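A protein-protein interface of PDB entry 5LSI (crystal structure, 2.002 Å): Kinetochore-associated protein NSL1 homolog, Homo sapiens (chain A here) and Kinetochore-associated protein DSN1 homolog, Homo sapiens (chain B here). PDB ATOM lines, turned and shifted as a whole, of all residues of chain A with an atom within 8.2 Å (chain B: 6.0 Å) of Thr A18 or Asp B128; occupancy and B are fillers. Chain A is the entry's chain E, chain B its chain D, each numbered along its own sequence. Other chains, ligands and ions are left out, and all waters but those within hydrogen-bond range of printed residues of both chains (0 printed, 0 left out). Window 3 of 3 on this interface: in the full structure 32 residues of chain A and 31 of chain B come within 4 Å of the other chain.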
ATOM      1  N   VAL A  15     -17.052 -24.134  24.995  1.00  0.00           N
ATOM      2  CA  VAL A  15     -17.627 -23.328  26.065  1.00  0.00           C
ATOM      3  C   VAL A  15     -18.548 -24.202  26.906  1.00  0.00           C
ATOM      4  O   VAL A  15     -19.454 -24.860  26.382  1.00  0.00           O
ATOM      5  CB  VAL A  15     -18.369 -22.116  25.485  1.00  0.00           C
ATOM      6  CG1 VAL A  15     -18.873 -21.212  26.601  1.00  0.00           C
ATOM      7  CG2 VAL A  15     -17.461 -21.351  24.537  1.00  0.00           C
ATOM      8  N   ARG A  16     -18.312 -24.220  28.216  1.00  0.00           N
ATOM      9  CA  ARG A  16     -19.012 -25.116  29.136  1.00  0.00           C
ATOM     10  C   ARG A  16     -20.333 -24.482  29.547  1.00  0.00           C
ATOM     11  O   ARG A  16     -20.377 -23.636  30.441  1.00  0.00           O
ATOM     12  CB  ARG A  16     -18.146 -25.410  30.357  1.00  0.00           C
ATOM     13  CG  ARG A  16     -16.988 -26.344  30.076  1.00  0.00           C
ATOM     14  CD  ARG A  16     -15.838 -26.134  31.046  1.00  0.00           C
ATOM     15  NE  ARG A  16     -14.748 -27.070  30.783  1.00  0.00           N
ATOM     16  CZ  ARG A  16     -13.548 -27.003  31.349  1.00  0.00           C
ATOM     17  NH1 ARG A  16     -13.272 -26.034  32.212  1.00  0.00           N
ATOM     18  NH2 ARG A  16     -12.622 -27.903  31.048  1.00  0.00           N
ATOM     19  N   CYS A  17     -21.419 -24.899  28.907  1.00  0.00           N
ATOM     20  CA  CYS A  17     -22.741 -24.371  29.198  1.00  0.00           C
ATOM     21  C   CYS A  17     -23.564 -25.398  29.963  1.00  0.00           C
ATOM     22  O   CYS A  17     -23.250 -26.592  29.983  1.00  0.00           O
ATOM     23  CB  CYS A  17     -23.466 -23.968  27.911  1.00  0.00           C
ATOM     24  SG  CYS A  17     -22.693 -22.579  27.054  1.00  0.00           S
ATOM     25  N   THR A  18     -24.631 -24.914  30.596  1.00  0.00           N
ATOM     26  CA  THR A  18     -25.505 -25.747  31.410  1.00  0.00           C
ATOM     27  C   THR A  18     -26.932 -25.840  30.893  1.00  0.00           C
ATOM     28  O   THR A  18     -27.597 -26.842  31.161  1.00  0.00           O
ATOM     29  CB  THR A  18     -25.553 -25.228  32.855  1.00  0.00           C
ATOM     30  OG1 THR A  18     -26.164 -23.932  32.878  1.00  0.00           O
ATOM     31  CG2 THR A  18     -24.153 -25.128  33.436  1.00  0.00           C
ATOM     32  N   SER A  19     -27.423 -24.834  30.170  1.00  0.00           N
ATOM     33  CA  SER A  19     -28.822 -24.774  29.756  1.00  0.00           C
ATOM     34  C   SER A  19     -28.911 -24.776  28.235  1.00  0.00           C
ATOM     35  O   SER A  19     -28.529 -23.800  27.581  1.00  0.00           O
ATOM     36  CB  SER A  19     -29.511 -23.540  30.335  1.00  0.00           C
ATOM     37  OG  SER A  19     -30.827 -23.432  29.828  1.00  0.00           O
ATOM     38  N   LYS A  20     -29.443 -25.866  27.680  1.00  0.00           N
ATOM     39  CA  LYS A  20     -29.660 -25.946  26.240  1.00  0.00           C
ATOM     40  C   LYS A  20     -30.706 -24.938  25.777  1.00  0.00           C
ATOM     41  O   LYS A  20     -30.577 -24.352  24.696  1.00  0.00           O
ATOM     42  CB  LYS A  20     -30.073 -27.370  25.871  1.00  0.00           C
ATOM     43  CG  LYS A  20     -29.910 -27.738  24.414  1.00  0.00           C
ATOM     44  CD  LYS A  20     -30.044 -29.244  24.237  1.00  0.00           C
ATOM     45  CE  LYS A  20     -30.126 -29.632  22.772  1.00  0.00           C
ATOM     46  NZ  LYS A  20     -30.197 -31.108  22.599  1.00  0.00           N
ATOM     47  N   ARG A  21     -31.752 -24.721  26.579  1.00  0.00           N
ATOM     48  CA  ARG A  21     -32.797 -23.786  26.177  1.00  0.00           C
ATOM     49  C   ARG A  21     -32.278 -22.355  26.134  1.00  0.00           C
ATOM     50  O   ARG A  21     -32.609 -21.599  25.216  1.00  0.00           O
ATOM     51  CB  ARG A  21     -33.992 -23.882  27.121  1.00  0.00           C
ATOM     52  CG  ARG A  21     -35.095 -22.891  26.795  1.00  0.00           C
ATOM     53  CD  ARG A  21     -36.178 -22.893  27.862  1.00  0.00           C
ATOM     54  NE  ARG A  21     -36.710 -24.232  28.100  1.00  0.00           N
ATOM     55  CZ  ARG A  21     -37.604 -24.525  29.038  1.00  0.00           C
ATOM     56  NH1 ARG A  21     -38.075 -23.571  29.833  1.00  0.00           N
ATOM     57  NH2 ARG A  21     -38.028 -25.774  29.183  1.00  0.00           N
ATOM     58  N   ALA A  22     -31.465 -21.968  27.120  1.00  0.00           N
ATOM     59  CA  ALA A  22     -30.938 -20.607  27.157  1.00  0.00           C
ATOM     60  C   ALA A  22     -30.032 -20.323  25.962  1.00  0.00           C
ATOM     61  O   ALA A  22     -30.021 -19.204  25.433  1.00  0.00           O
ATOM     62  CB  ALA A  22     -30.191 -20.375  28.471  1.00  0.00           C
ATOM     63  N   VAL A  23     -29.260 -21.320  25.525  1.00  0.00           N
ATOM     64  CA  VAL A  23     -28.450 -21.151  24.322  1.00  0.00           C
ATOM     65  C   VAL A  23     -29.345 -20.976  23.102  1.00  0.00           C
ATOM     66  O   VAL A  23     -29.094 -20.114  22.248  1.00  0.00           O
ATOM     67  CB  VAL A  23     -27.486 -22.340  24.151  1.00  0.00           C
ATOM     68  CG1 VAL A  23     -26.738 -22.241  22.824  1.00  0.00           C
ATOM     69  CG2 VAL A  23     -26.510 -22.408  25.314  1.00  0.00           C
ATOM     70  N   ILE A  65     -19.859 -25.788  21.993  1.00  0.00           N
ATOM     71  CA  ILE A  65     -20.219 -25.739  23.402  1.00  0.00           C
ATOM     72  C   ILE A  65     -20.491 -27.160  23.870  1.00  0.00           C
ATOM     73  O   ILE A  65     -20.733 -28.070  23.074  1.00  0.00           O
ATOM     74  CB  ILE A  65     -21.447 -24.840  23.690  1.00  0.00           C
ATOM     75  CG1 ILE A  65     -22.740 -25.517  23.233  1.00  0.00           C
ATOM     76  CG2 ILE A  65     -21.306 -23.485  23.021  1.00  0.00           C
ATOM     77  CD1 ILE A  65     -23.974 -24.650  23.409  1.00  0.00           C
ATOM     78  N   SER A  66     -20.431 -27.343  25.181  1.00  0.00           N
ATOM     79  CA  SER A  66     -20.903 -28.555  25.825  1.00  0.00           C
ATOM     80  C   SER A  66     -22.065 -28.199  26.741  1.00  0.00           C
ATOM     81  O   SER A  66     -22.110 -27.109  27.318  1.00  0.00           O
ATOM     82  CB  SER A  66     -19.788 -29.243  26.624  1.00  0.00           C
ATOM     83  OG  SER A  66     -19.279 -28.384  27.631  1.00  0.00           O
ATOM     84  N   ILE A  67     -23.017 -29.117  26.854  1.00  0.00           N
ATOM     85  CA  ILE A  67     -24.152 -28.967  27.756  1.00  0.00           C
ATOM     86  C   ILE A  67     -23.922 -29.939  28.904  1.00  0.00           C
ATOM     87  O   ILE A  67     -24.144 -31.148  28.761  1.00  0.00           O
ATOM     88  CB  ILE A  67     -25.488 -29.225  27.053  1.00  0.00           C
ATOM     89  CG1 ILE A  67     -25.676 -28.252  25.887  1.00  0.00           C
ATOM     90  CG2 ILE A  67     -26.648 -29.108  28.041  1.00  0.00           C
ATOM     91  CD1 ILE A  67     -25.693 -26.801  26.303  1.00  0.00           C
ATOM     92  N   ASN A  68     -23.466 -29.413  30.043  1.00  0.00           N
ATOM     93  CA  ASN A  68     -23.111 -30.226  31.208  1.00  0.00           C
ATOM     94  C   ASN A  68     -22.087 -31.296  30.829  1.00  0.00           C
ATOM     95  O   ASN A  68     -22.261 -32.486  31.101  1.00  0.00           O
ATOM     96  CB  ASN A  68     -24.356 -30.847  31.847  1.00  0.00           C
ATOM     97  CG  ASN A  68     -25.307 -29.805  32.406  1.00  0.00           C
ATOM     98  OD1 ASN A  68     -24.894 -28.884  33.112  1.00  0.00           O
ATOM     99  ND2 ASN A  68     -26.588 -29.941  32.085  1.00  0.00           N
ATOM    100  N   GLY A  69     -21.011 -30.857  30.173  1.00  0.00           N
ATOM    101  CA  GLY A  69     -19.948 -31.744  29.750  1.00  0.00           C
ATOM    102  C   GLY A  69     -20.275 -32.652  28.585  1.00  0.00           C
ATOM    103  O   GLY A  69     -19.388 -33.386  28.131  1.00  0.00           O
ATOM    104  N   ALA A  75     -27.478 -34.100  24.654  1.00  0.00           N
ATOM    105  CA  ALA A  75     -27.936 -33.550  25.921  1.00  0.00           C
ATOM    106  C   ALA A  75     -29.383 -33.080  25.795  1.00  0.00           C
ATOM    107  O   ALA A  75     -30.014 -33.190  24.739  1.00  0.00           O
ATOM    108  CB  ALA A  75     -27.022 -32.410  26.373  1.00  0.00           C
ATOM    109  N   SER A  76     -29.909 -32.547  26.892  1.00  0.00           N
ATOM    110  CA  SER A  76     -31.297 -32.109  26.933  1.00  0.00           C
ATOM    111  C   SER A  76     -31.446 -30.799  27.703  1.00  0.00           C
ATOM    112  O   SER A  76     -30.977 -30.678  28.834  1.00  0.00           O
ATOM    113  CB  SER A  76     -32.176 -33.192  27.561  1.00  0.00           C
ATOM    114  OG  SER A  76     -31.971 -34.443  26.924  1.00  0.00           O
ATOM    115  N   LYS B 124     -27.449 -16.720  31.663  1.00  0.00           N
ATOM    116  CA  LYS B 124     -28.444 -17.780  31.782  1.00  0.00           C
ATOM    117  C   LYS B 124     -27.975 -19.091  31.163  1.00  0.00           C
ATOM    118  O   LYS B 124     -28.441 -20.157  31.578  1.00  0.00           O
ATOM    119  CB  LYS B 124     -29.759 -17.347  31.136  1.00  0.00           C
ATOM    120  CG  LYS B 124     -30.489 -16.233  31.867  1.00  0.00           C
ATOM    121  CD  LYS B 124     -31.829 -15.956  31.203  1.00  0.00           C
ATOM    122  CE  LYS B 124     -32.660 -14.970  32.004  1.00  0.00           C
ATOM    123  NZ  LYS B 124     -34.034 -14.839  31.445  1.00  0.00           N
ATOM    124  N   CYS B 125     -27.061 -19.040  30.188  1.00  0.00           N
ATOM    125  CA  CYS B 125     -26.531 -20.260  29.592  1.00  0.00           C
ATOM    126  C   CYS B 125     -25.667 -21.058  30.557  1.00  0.00           C
ATOM    127  O   CYS B 125     -25.341 -22.213  30.261  1.00  0.00           O
ATOM    128  CB  CYS B 125     -25.719 -19.927  28.340  1.00  0.00           C
ATOM    129  SG  CYS B 125     -26.641 -19.060  27.058  1.00  0.00           S
ATOM    130  N   PHE B 126     -25.286 -20.474  31.691  1.00  0.00           N
ATOM    131  CA  PHE B 126     -24.408 -21.126  32.648  1.00  0.00           C
ATOM    132  C   PHE B 126     -25.079 -21.379  33.986  1.00  0.00           C
ATOM    133  O   PHE B 126     -24.416 -21.847  34.916  1.00  0.00           O
ATOM    134  CB  PHE B 126     -23.141 -20.287  32.855  1.00  0.00           C
ATOM    135  CG  PHE B 126     -22.423 -19.963  31.578  1.00  0.00           C
ATOM    136  CD1 PHE B 126     -21.464 -20.822  31.072  1.00  0.00           C
ATOM    137  CD2 PHE B 126     -22.719 -18.806  30.875  1.00  0.00           C
ATOM    138  CE1 PHE B 126     -20.808 -20.533  29.892  1.00  0.00           C
ATOM    139  CE2 PHE B 126     -22.064 -18.508  29.694  1.00  0.00           C
ATOM    140  CZ  PHE B 126     -21.107 -19.373  29.202  1.00  0.00           C
ATOM    141  N   GLU B 127     -26.366 -21.089  34.109  1.00  0.00           N
ATOM    142  CA  GLU B 127     -27.107 -21.312  35.339  1.00  0.00           C
ATOM    143  C   GLU B 127     -27.972 -22.557  35.209  1.00  0.00           C
ATOM    144  O   GLU B 127     -28.468 -22.882  34.127  1.00  0.00           O
ATOM    145  CB  GLU B 127     -27.987 -20.107  35.671  1.00  0.00           C
ATOM    146  CG  GLU B 127     -27.215 -18.872  36.098  1.00  0.00           C
ATOM    147  CD  GLU B 127     -28.039 -17.603  35.974  1.00  0.00           C
ATOM    148  OE1 GLU B 127     -29.202 -17.686  35.524  1.00  0.00           O
ATOM    149  OE2 GLU B 127     -27.526 -16.523  36.332  1.00  0.00           O
ATOM    150  N   ASP B 128     -28.143 -23.255  36.327  1.00  0.00           N
ATOM    151  CA  ASP B 128     -29.102 -24.347  36.390  1.00  0.00           C
ATOM    152  C   ASP B 128     -29.715 -24.386  37.779  1.00  0.00           C
ATOM    153  O   ASP B 128     -28.998 -24.383  38.783  1.00  0.00           O
ATOM    154  CB  ASP B 128     -28.459 -25.700  36.043  1.00  0.00           C
ATOM    155  CG  ASP B 128     -27.165 -25.957  36.798  1.00  0.00           C
ATOM    156  OD1 ASP B 128     -27.224 -26.275  38.005  1.00  0.00           O
ATOM    157  OD2 ASP B 128     -26.085 -25.856  36.177  1.00  0.00           O
ATOM    158  N   SER B 129     -31.041 -24.377  37.823  1.00  0.00           N
ATOM    159  CA  SER B 129     -31.824 -24.681  39.013  1.00  0.00           C
ATOM    160  C   SER B 129     -32.976 -25.592  38.621  1.00  0.00           C
ATOM    161  O   SER B 129     -34.132 -25.383  38.992  1.00  0.00           O
ATOM    162  CB  SER B 129     -32.324 -23.406  39.691  1.00  0.00           C
ATOM    163  OG  SER B 129     -32.543 -23.613  41.076  1.00  0.00           O
ATOM    164  N   ASN B 130     -32.653 -26.618  37.834  1.00  0.00           N
ATOM    165  CA  ASN B 130     -33.626 -27.483  37.180  1.00  0.00           C
ATOM    166  C   ASN B 130     -33.343 -28.936  37.549  1.00  0.00           C
ATOM    167  O   ASN B 130     -32.375 -29.252  38.246  1.00  0.00           O
ATOM    168  CB  ASN B 130     -33.586 -27.301  35.655  1.00  0.00           C
ATOM    169  CG  ASN B 130     -33.799 -25.858  35.227  1.00  0.00           C
ATOM    170  OD1 ASN B 130     -34.935 -25.409  35.059  1.00  0.00           O
ATOM    171  ND2 ASN B 130     -32.703 -25.125  35.042  1.00  0.00           N
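Of chain B, only Cys B125 (2.8 Å), Phe B126 (3.0 Å), Glu B127 (2.8 Å) and Asp B128 (3.4 Å) come within 4 Å of Thr A18.
Asp B128 touches just one residue of chain A: Thr A18 (3.4 Å).
Of the printed residues of chain B, Val A15 touches Phe B126 (3.9 Å).
Of the printed residues of chain B, Val A23 touches Cys B125.
Of the printed residues of chain B, Arg A16 touches Phe B126 (3.1 Å).
The nearest residue of chain A that does not touch Asp B128 is Asn A68 (4.5 Å).
The nearest printed residue of chain B that does not touch Ser A19 is Phe B126 (5.1 Å).
The backbone carbonyl oxygen (O) of Val A15 lies within hydrogen-bond range of the backbone NH (N) of Ser A66 (2.9 Å).
N of Cys A17 lies within hydrogen-bond range of O of Ser A66, at 2.8 Å.
The backbone carbonyl oxygen (O) of Cys A17 sits at hydrogen-bond distance from the backbone NH (N) of Asn A68, 2.8 Å away.
The backbone carbonyl oxygen of Thr A18 sits at hydrogen-bond distance from the side-chain amide nitrogen of Asn A68.
OG of Ser A19 sits at hydrogen-bond distance from N of Ala A22, 3.1 Å away.
Among the printed residues, pairs that only touch across the chains: Val A15 with Phe B126 (3.9 Å), Arg A16 with Phe B126 (3.1 Å), Cys A17 with Cys B125 (3.5 Å), Cys A17 with Phe B126 (3.97 Å), Thr A18 with Asp B128 (3.4 Å), Ser A19 with Lys B124 (3.8 Å), Ser A19 with Glu B127 (3.99 Å) and Ala A22 with Lys B124 (3.6 Å).
Of the 16 printed residues of chain A, 7 touch a printed residue of chain B.
Printed residues of chain A that touch a printed residue of chain B: Val A15, Arg A16, Cys A17, Thr A18, Ser A19, Ala A22 and Val A23.
Of the 7 printed residues of chain B, 5 touch a printed residue of chain A.
Among the printed residues, no Asp or Glu carboxylate lies within 4 Å of a Lys or Arg side-chain nitrogen of the other chain.
The backbone NH (N) of Thr A18 sits at hydrogen-bond distance from the backbone carbonyl oxygen (O) of Cys B125, at 2.8 Å.
O of Cys B125 sits at hydrogen-bond distance from N of Ser A19, at 3.3 Å.
The side-chain sulfur of Cys B125 sits at hydrogen-bond distance from the backbone carbonyl oxygen of Ala A22 (3.8 Å).
N of Val A23 sits close to SG of Cys B125 (3.8 Å).
The backbone carbonyl oxygen of Phe B126 sits close to the side-chain hydroxyl of Thr A18, at 3.4 Å.
The backbone carbonyl oxygen (O) of Glu B127 sits at hydrogen-bond distance from the side-chain hydroxyl (OG1) of Thr A18, at 2.8 Å.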
